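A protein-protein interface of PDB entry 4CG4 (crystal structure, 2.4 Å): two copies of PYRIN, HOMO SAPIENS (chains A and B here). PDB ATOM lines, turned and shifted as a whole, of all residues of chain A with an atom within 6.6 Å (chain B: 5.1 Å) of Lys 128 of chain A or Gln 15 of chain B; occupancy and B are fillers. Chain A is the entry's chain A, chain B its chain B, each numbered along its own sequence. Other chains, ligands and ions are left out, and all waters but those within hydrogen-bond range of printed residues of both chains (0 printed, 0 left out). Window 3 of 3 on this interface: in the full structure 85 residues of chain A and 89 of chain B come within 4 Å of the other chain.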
ATOM      1  N   LEU A 101     -15.628 -33.103 -11.702  1.00  0.00           N
ATOM      2  CA  LEU A 101     -14.326 -32.439 -11.823  1.00  0.00           C
ATOM      3  C   LEU A 101     -14.161 -31.415 -10.697  1.00  0.00           C
ATOM      4  O   LEU A 101     -13.099 -31.328 -10.063  1.00  0.00           O
ATOM      5  CB  LEU A 101     -14.183 -31.770 -13.195  1.00  0.00           C
ATOM      6  CG  LEU A 101     -14.034 -32.710 -14.410  1.00  0.00           C
ATOM      7  CD1 LEU A 101     -14.004 -31.947 -15.731  1.00  0.00           C
ATOM      8  CD2 LEU A 101     -12.783 -33.556 -14.297  1.00  0.00           C
ATOM      9  N   ILE A 102     -15.216 -30.651 -10.434  1.00  0.00           N
ATOM     10  CA  ILE A 102     -15.210 -29.727  -9.300  1.00  0.00           C
ATOM     11  C   ILE A 102     -14.913 -30.491  -8.000  1.00  0.00           C
ATOM     12  O   ILE A 102     -14.115 -30.034  -7.183  1.00  0.00           O
ATOM     13  CB  ILE A 102     -16.567 -28.948  -9.187  1.00  0.00           C
ATOM     14  CG1 ILE A 102     -16.702 -27.971 -10.354  1.00  0.00           C
ATOM     15  CG2 ILE A 102     -16.643 -28.129  -7.893  1.00  0.00           C
ATOM     16  CD1 ILE A 102     -18.099 -27.487 -10.607  1.00  0.00           C
ATOM     17  N   LEU A 105     -11.130 -31.419  -7.906  1.00  0.00           N
ATOM     18  CA  LEU A 105     -10.276 -30.273  -7.640  1.00  0.00           C
ATOM     19  C   LEU A 105     -10.389 -29.814  -6.196  1.00  0.00           C
ATOM     20  O   LEU A 105      -9.377 -29.507  -5.530  1.00  0.00           O
ATOM     21  CB  LEU A 105     -10.609 -29.131  -8.579  1.00  0.00           C
ATOM     22  CG  LEU A 105     -10.141 -29.351 -10.015  1.00  0.00           C
ATOM     23  CD1 LEU A 105     -10.641 -28.225 -10.891  1.00  0.00           C
ATOM     24  CD2 LEU A 105      -8.610 -29.474 -10.121  1.00  0.00           C
ATOM     25  N   ILE A 123      -6.022 -34.260 -13.914  1.00  0.00           N
ATOM     26  CA  ILE A 123      -7.239 -33.584 -13.499  1.00  0.00           C
ATOM     27  C   ILE A 123      -7.295 -32.195 -14.136  1.00  0.00           C
ATOM     28  O   ILE A 123      -8.349 -31.824 -14.702  1.00  0.00           O
ATOM     29  CB  ILE A 123      -7.374 -33.507 -11.937  1.00  0.00           C
ATOM     30  CG1 ILE A 123      -8.653 -32.772 -11.543  1.00  0.00           C
ATOM     31  CG2 ILE A 123      -6.231 -32.788 -11.304  1.00  0.00           C
ATOM     32  CD1 ILE A 123      -9.924 -33.469 -12.017  1.00  0.00           C
ATOM     33  N   LEU A 124      -6.187 -31.446 -14.068  1.00  0.00           N
ATOM     34  CA  LEU A 124      -6.148 -30.098 -14.655  1.00  0.00           C
ATOM     35  C   LEU A 124      -6.312 -30.129 -16.169  1.00  0.00           C
ATOM     36  O   LEU A 124      -6.993 -29.266 -16.747  1.00  0.00           O
ATOM     37  CB  LEU A 124      -4.866 -29.364 -14.289  1.00  0.00           C
ATOM     38  CG  LEU A 124      -4.745 -28.932 -12.827  1.00  0.00           C
ATOM     39  CD1 LEU A 124      -3.324 -28.463 -12.527  1.00  0.00           C
ATOM     40  CD2 LEU A 124      -5.737 -27.844 -12.472  1.00  0.00           C
ATOM     41  N   HIS A 125      -5.677 -31.090 -16.832  1.00  0.00           N
ATOM     42  CA  HIS A 125      -5.897 -31.190 -18.267  1.00  0.00           C
ATOM     43  C   HIS A 125      -7.376 -31.399 -18.581  1.00  0.00           C
ATOM     44  O   HIS A 125      -7.935 -30.758 -19.473  1.00  0.00           O
ATOM     45  CB  HIS A 125      -5.118 -32.332 -18.888  1.00  0.00           C
ATOM     46  CG  HIS A 125      -5.435 -32.519 -20.337  1.00  0.00           C
ATOM     47  ND1 HIS A 125      -5.051 -31.611 -21.300  1.00  0.00           N
ATOM     48  CD2 HIS A 125      -6.150 -33.471 -20.980  1.00  0.00           C
ATOM     49  CE1 HIS A 125      -5.492 -32.011 -22.482  1.00  0.00           C
ATOM     50  NE2 HIS A 125      -6.160 -33.137 -22.314  1.00  0.00           N
ATOM     51  N   ARG A 126      -7.986 -32.330 -17.858  1.00  0.00           N
ATOM     52  CA  ARG A 126      -9.382 -32.647 -18.050  1.00  0.00           C
ATOM     53  C   ARG A 126     -10.287 -31.470 -17.694  1.00  0.00           C
ATOM     54  O   ARG A 126     -11.341 -31.276 -18.318  1.00  0.00           O
ATOM     55  CB  ARG A 126      -9.742 -33.894 -17.257  1.00  0.00           C
ATOM     56  CG  ARG A 126      -9.193 -35.138 -17.933  1.00  0.00           C
ATOM     57  CD  ARG A 126      -9.577 -36.452 -17.256  1.00  0.00           C
ATOM     58  NE  ARG A 126      -9.024 -36.564 -15.914  1.00  0.00           N
ATOM     59  CZ  ARG A 126      -9.737 -36.512 -14.795  1.00  0.00           C
ATOM     60  NH1 ARG A 126     -11.058 -36.354 -14.836  1.00  0.00           N
ATOM     61  NH2 ARG A 126      -9.116 -36.620 -13.629  1.00  0.00           N
ATOM     62  N   ALA A 127      -9.892 -30.679 -16.702  1.00  0.00           N
ATOM     63  CA  ALA A 127     -10.665 -29.480 -16.373  1.00  0.00           C
ATOM     64  C   ALA A 127     -10.613 -28.461 -17.527  1.00  0.00           C
ATOM     65  O   ALA A 127     -11.654 -27.968 -17.989  1.00  0.00           O
ATOM     66  CB  ALA A 127     -10.151 -28.873 -15.103  1.00  0.00           C
ATOM     67  N   LYS A 128      -9.399 -28.203 -18.005  1.00  0.00           N
ATOM     68  CA  LYS A 128      -9.141 -27.287 -19.112  1.00  0.00           C
ATOM     69  C   LYS A 128      -9.887 -27.631 -20.377  1.00  0.00           C
ATOM     70  O   LYS A 128     -10.242 -26.755 -21.149  1.00  0.00           O
ATOM     71  CB  LYS A 128      -7.641 -27.304 -19.447  1.00  0.00           C
ATOM     72  CG  LYS A 128      -7.160 -26.274 -20.466  1.00  0.00           C
ATOM     73  CD  LYS A 128      -5.664 -26.462 -20.753  1.00  0.00           C
ATOM     74  CE  LYS A 128      -5.209 -25.613 -21.930  1.00  0.00           C
ATOM     75  NZ  LYS A 128      -3.733 -25.456 -21.976  1.00  0.00           N
ATOM     76  N   THR A 129     -10.107 -28.918 -20.592  1.00  0.00           N
ATOM     77  CA  THR A 129     -10.658 -29.399 -21.850  1.00  0.00           C
ATOM     78  C   THR A 129     -12.122 -29.878 -21.773  1.00  0.00           C
ATOM     79  O   THR A 129     -12.658 -30.417 -22.743  1.00  0.00           O
ATOM     80  CB  THR A 129      -9.780 -30.548 -22.398  1.00  0.00           C
ATOM     81  OG1 THR A 129      -9.666 -31.576 -21.408  1.00  0.00           O
ATOM     82  CG2 THR A 129      -8.397 -30.029 -22.735  1.00  0.00           C
ATOM     83  N   VAL A 130     -12.785 -29.684 -20.645  1.00  0.00           N
ATOM     84  CA  VAL A 130     -14.156 -30.157 -20.558  1.00  0.00           C
ATOM     85  C   VAL A 130     -15.049 -29.318 -21.503  1.00  0.00           C
ATOM     86  O   VAL A 130     -14.922 -28.101 -21.558  1.00  0.00           O
ATOM     87  CB  VAL A 130     -14.668 -30.102 -19.110  1.00  0.00           C
ATOM     88  CG1 VAL A 130     -14.923 -28.660 -18.681  1.00  0.00           C
ATOM     89  CG2 VAL A 130     -15.906 -30.918 -18.984  1.00  0.00           C
ATOM     90  N   LYS B  11      -3.460 -22.705 -10.270  1.00  0.00           N
ATOM     91  CA  LYS B  11      -4.194 -23.266 -11.396  1.00  0.00           C
ATOM     92  C   LYS B  11      -5.483 -24.008 -10.965  1.00  0.00           C
ATOM     93  O   LYS B  11      -6.478 -24.017 -11.711  1.00  0.00           O
ATOM     94  CB  LYS B  11      -3.283 -24.164 -12.239  1.00  0.00           C
ATOM     95  CG  LYS B  11      -2.172 -23.374 -12.995  1.00  0.00           C
ATOM     96  CD  LYS B  11      -2.681 -22.154 -13.833  1.00  0.00           C
ATOM     97  CE  LYS B  11      -3.214 -22.520 -15.221  1.00  0.00           C
ATOM     98  NZ  LYS B  11      -3.444 -21.300 -16.065  1.00  0.00           N
ATOM     99  N   ILE B  12      -5.471 -24.660  -9.804  1.00  0.00           N
ATOM    100  CA  ILE B  12      -6.691 -25.293  -9.326  1.00  0.00           C
ATOM    101  C   ILE B  12      -7.782 -24.218  -9.141  1.00  0.00           C
ATOM    102  O   ILE B  12      -8.896 -24.394  -9.651  1.00  0.00           O
ATOM    103  CB  ILE B  12      -6.473 -26.073  -8.024  1.00  0.00           C
ATOM    104  CG1 ILE B  12      -5.686 -27.359  -8.302  1.00  0.00           C
ATOM    105  CG2 ILE B  12      -7.829 -26.428  -7.380  1.00  0.00           C
ATOM    106  CD1 ILE B  12      -5.160 -28.026  -7.040  1.00  0.00           C
ATOM    107  N   GLN B  13      -7.461 -23.106  -8.463  1.00  0.00           N
ATOM    108  CA  GLN B  13      -8.455 -22.033  -8.286  1.00  0.00           C
ATOM    109  C   GLN B  13      -8.993 -21.526  -9.610  1.00  0.00           C
ATOM    110  O   GLN B  13     -10.227 -21.400  -9.811  1.00  0.00           O
ATOM    111  CB  GLN B  13      -7.880 -20.852  -7.502  1.00  0.00           C
ATOM    112  CG  GLN B  13      -7.843 -21.080  -5.997  1.00  0.00           C
ATOM    113  CD  GLN B  13      -9.219 -21.417  -5.423  1.00  0.00           C
ATOM    114  OE1 GLN B  13      -9.414 -22.473  -4.819  1.00  0.00           O
ATOM    115  NE2 GLN B  13     -10.177 -20.514  -5.613  1.00  0.00           N
ATOM    116  N   LYS B  14      -8.075 -21.252 -10.523  1.00  0.00           N
ATOM    117  CA  LYS B  14      -8.494 -20.807 -11.839  1.00  0.00           C
ATOM    118  C   LYS B  14      -9.495 -21.814 -12.471  1.00  0.00           C
ATOM    119  O   LYS B  14     -10.607 -21.431 -12.894  1.00  0.00           O
ATOM    120  CB  LYS B  14      -7.273 -20.607 -12.735  1.00  0.00           C
ATOM    121  CG  LYS B  14      -7.599 -20.132 -14.122  1.00  0.00           C
ATOM    122  CD  LYS B  14      -6.381 -20.140 -15.014  1.00  0.00           C
ATOM    123  CE  LYS B  14      -6.764 -19.763 -16.424  1.00  0.00           C
ATOM    124  NZ  LYS B  14      -5.599 -19.836 -17.341  1.00  0.00           N
ATOM    125  N   GLN B  15      -9.124 -23.091 -12.511  1.00  0.00           N
ATOM    126  CA  GLN B  15      -9.982 -24.077 -13.142  1.00  0.00           C
ATOM    127  C   GLN B  15     -11.318 -24.234 -12.412  1.00  0.00           C
ATOM    128  O   GLN B  15     -12.342 -24.480 -13.045  1.00  0.00           O
ATOM    129  CB  GLN B  15      -9.280 -25.424 -13.229  1.00  0.00           C
ATOM    130  CG  GLN B  15      -8.083 -25.451 -14.167  1.00  0.00           C
ATOM    131  CD  GLN B  15      -8.395 -24.903 -15.548  1.00  0.00           C
ATOM    132  OE1 GLN B  15      -9.500 -25.076 -16.080  1.00  0.00           O
ATOM    133  NE2 GLN B  15      -7.416 -24.236 -16.139  1.00  0.00           N
ATOM    134  N   LEU B  16     -11.309 -24.090 -11.090  1.00  0.00           N
ATOM    135  CA  LEU B  16     -12.547 -24.114 -10.334  1.00  0.00           C
ATOM    136  C   LEU B  16     -13.477 -23.019 -10.811  1.00  0.00           C
ATOM    137  O   LEU B  16     -14.673 -23.261 -11.029  1.00  0.00           O
ATOM    138  CB  LEU B  16     -12.272 -23.958  -8.850  1.00  0.00           C
ATOM    139  CG  LEU B  16     -12.027 -25.270  -8.107  1.00  0.00           C
ATOM    140  CD1 LEU B  16     -11.359 -24.990  -6.783  1.00  0.00           C
ATOM    141  CD2 LEU B  16     -13.342 -26.000  -7.879  1.00  0.00           C
ATOM    142  N   GLU B  17     -12.947 -21.814 -10.978  1.00  0.00           N
ATOM    143  CA  GLU B  17     -13.787 -20.744 -11.502  1.00  0.00           C
ATOM    144  C   GLU B  17     -14.358 -21.060 -12.856  1.00  0.00           C
ATOM    145  O   GLU B  17     -15.587 -20.945 -13.093  1.00  0.00           O
ATOM    146  CB  GLU B  17     -13.039 -19.436 -11.608  1.00  0.00           C
ATOM    147  CG  GLU B  17     -12.993 -18.684 -10.329  1.00  0.00           C
ATOM    148  CD  GLU B  17     -12.308 -17.371 -10.502  1.00  0.00           C
ATOM    149  OE1 GLU B  17     -11.253 -17.347 -11.176  1.00  0.00           O
ATOM    150  OE2 GLU B  17     -12.846 -16.361  -9.990  1.00  0.00           O
ATOM    151  N   HIS B  18     -13.479 -21.487 -13.746  1.00  0.00           N
ATOM    152  CA  HIS B  18     -13.943 -21.894 -15.077  1.00  0.00           C
ATOM    153  C   HIS B  18     -15.112 -22.895 -15.010  1.00  0.00           C
ATOM    154  O   HIS B  18     -16.151 -22.704 -15.653  1.00  0.00           O
ATOM    155  CB  HIS B  18     -12.812 -22.516 -15.867  1.00  0.00           C
ATOM    156  CG  HIS B  18     -13.200 -22.912 -17.251  1.00  0.00           C
ATOM    157  ND1 HIS B  18     -13.586 -21.995 -18.201  1.00  0.00           N
ATOM    158  CD2 HIS B  18     -13.262 -24.130 -17.844  1.00  0.00           C
ATOM    159  CE1 HIS B  18     -13.870 -22.630 -19.329  1.00  0.00           C
ATOM    160  NE2 HIS B  18     -13.682 -23.922 -19.137  1.00  0.00           N
ATOM    161  N   LEU B  19     -14.902 -23.968 -14.252  1.00  0.00           N
ATOM    162  CA  LEU B  19     -15.849 -25.047 -14.208  1.00  0.00           C
ATOM    163  C   LEU B  19     -17.176 -24.559 -13.647  1.00  0.00           C
ATOM    164  O   LEU B  19     -18.237 -24.904 -14.188  1.00  0.00           O
ATOM    165  CB  LEU B  19     -15.318 -26.210 -13.374  1.00  0.00           C
ATOM    166  CG  LEU B  19     -14.093 -26.961 -13.892  1.00  0.00           C
ATOM    167  CD1 LEU B  19     -13.669 -28.001 -12.857  1.00  0.00           C
ATOM    168  CD2 LEU B  19     -14.362 -27.602 -15.241  1.00  0.00           C
ATOM    169  N   LYS B  20     -17.110 -23.730 -12.605  1.00  0.00           N
ATOM    170  CA  LYS B  20     -18.323 -23.209 -12.011  1.00  0.00           C
ATOM    171  C   LYS B  20     -19.129 -22.344 -12.991  1.00  0.00           C
ATOM    172  O   LYS B  20     -20.362 -22.521 -13.089  1.00  0.00           O
ATOM    173  CB  LYS B  20     -18.007 -22.460 -10.721  1.00  0.00           C
ATOM    174  CG  LYS B  20     -17.873 -23.454  -9.594  1.00  0.00           C
ATOM    175  CD  LYS B  20     -17.216 -22.931  -8.351  1.00  0.00           C
ATOM    176  CE  LYS B  20     -17.116 -24.051  -7.292  1.00  0.00           C
ATOM    177  NZ  LYS B  20     -16.376 -23.678  -6.047  1.00  0.00           N
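Among the printed residues, merely in contact across the chains: Leu 101 of chain A with Leu 19 of chain B (3.8 Å), Ile 102 of chain A with Leu 16 of chain B (3.9 Å), Ile 102 of chain A with Leu 19 of chain B (3.8 Å), Leu 105 of chain A with Ile 12 of chain B (3.9 Å), Leu 105 of chain A with Gln 15 of chain B (3.9 Å), Leu 105 of chain A with Leu 19 of chain B (3.6 Å), Leu 124 of chain A with Lys 11 of chain B (3.97 Å), Leu 124 of chain A with Gln 15 of chain B (3.8 Å), Ala 127 of chain A with Gln 15 of chain B (3.8 Å), Ala 127 of chain A with Leu 19 of chain B (3.9 Å), Lys 128 of chain A with Gln 15 of chain B (3.7 Å) and Val 130 of chain A with Leu 19 of chain B (3.6 Å).
Of chain B, only Gln 15 comes within 4 Å of Lys 128 of chain A.
Of chain A, only Leu 105 (3.9 Å), Leu 124 (3.8 Å), Ala 127 (3.8 Å) and Lys 128 (3.7 Å) come within 4 Å of Gln 15 of chain B.
Of the printed residues of chain B, Leu 124 of chain A touches Lys 11 and Gln 15.
Printed residues of chain B within 4 Å of Leu 105 of chain A: Ile 12 (3.9 Å), Gln 15 (3.9 Å) and Leu 19 (3.6 Å).
Thr 129 of chain A touches none of the printed residues of chain B.
The nearest residue of chain B that does not touch Lys 128 of chain A is His 18 of chain B (4.9 Å).
The nearest printed residue of chain B that does not touch Leu 124 of chain A is Ile 12 of chain B (4.2 Å).
Of the 11 printed residues of chain A, 7 touch a printed residue of chain B.
No position is printed for both chains.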
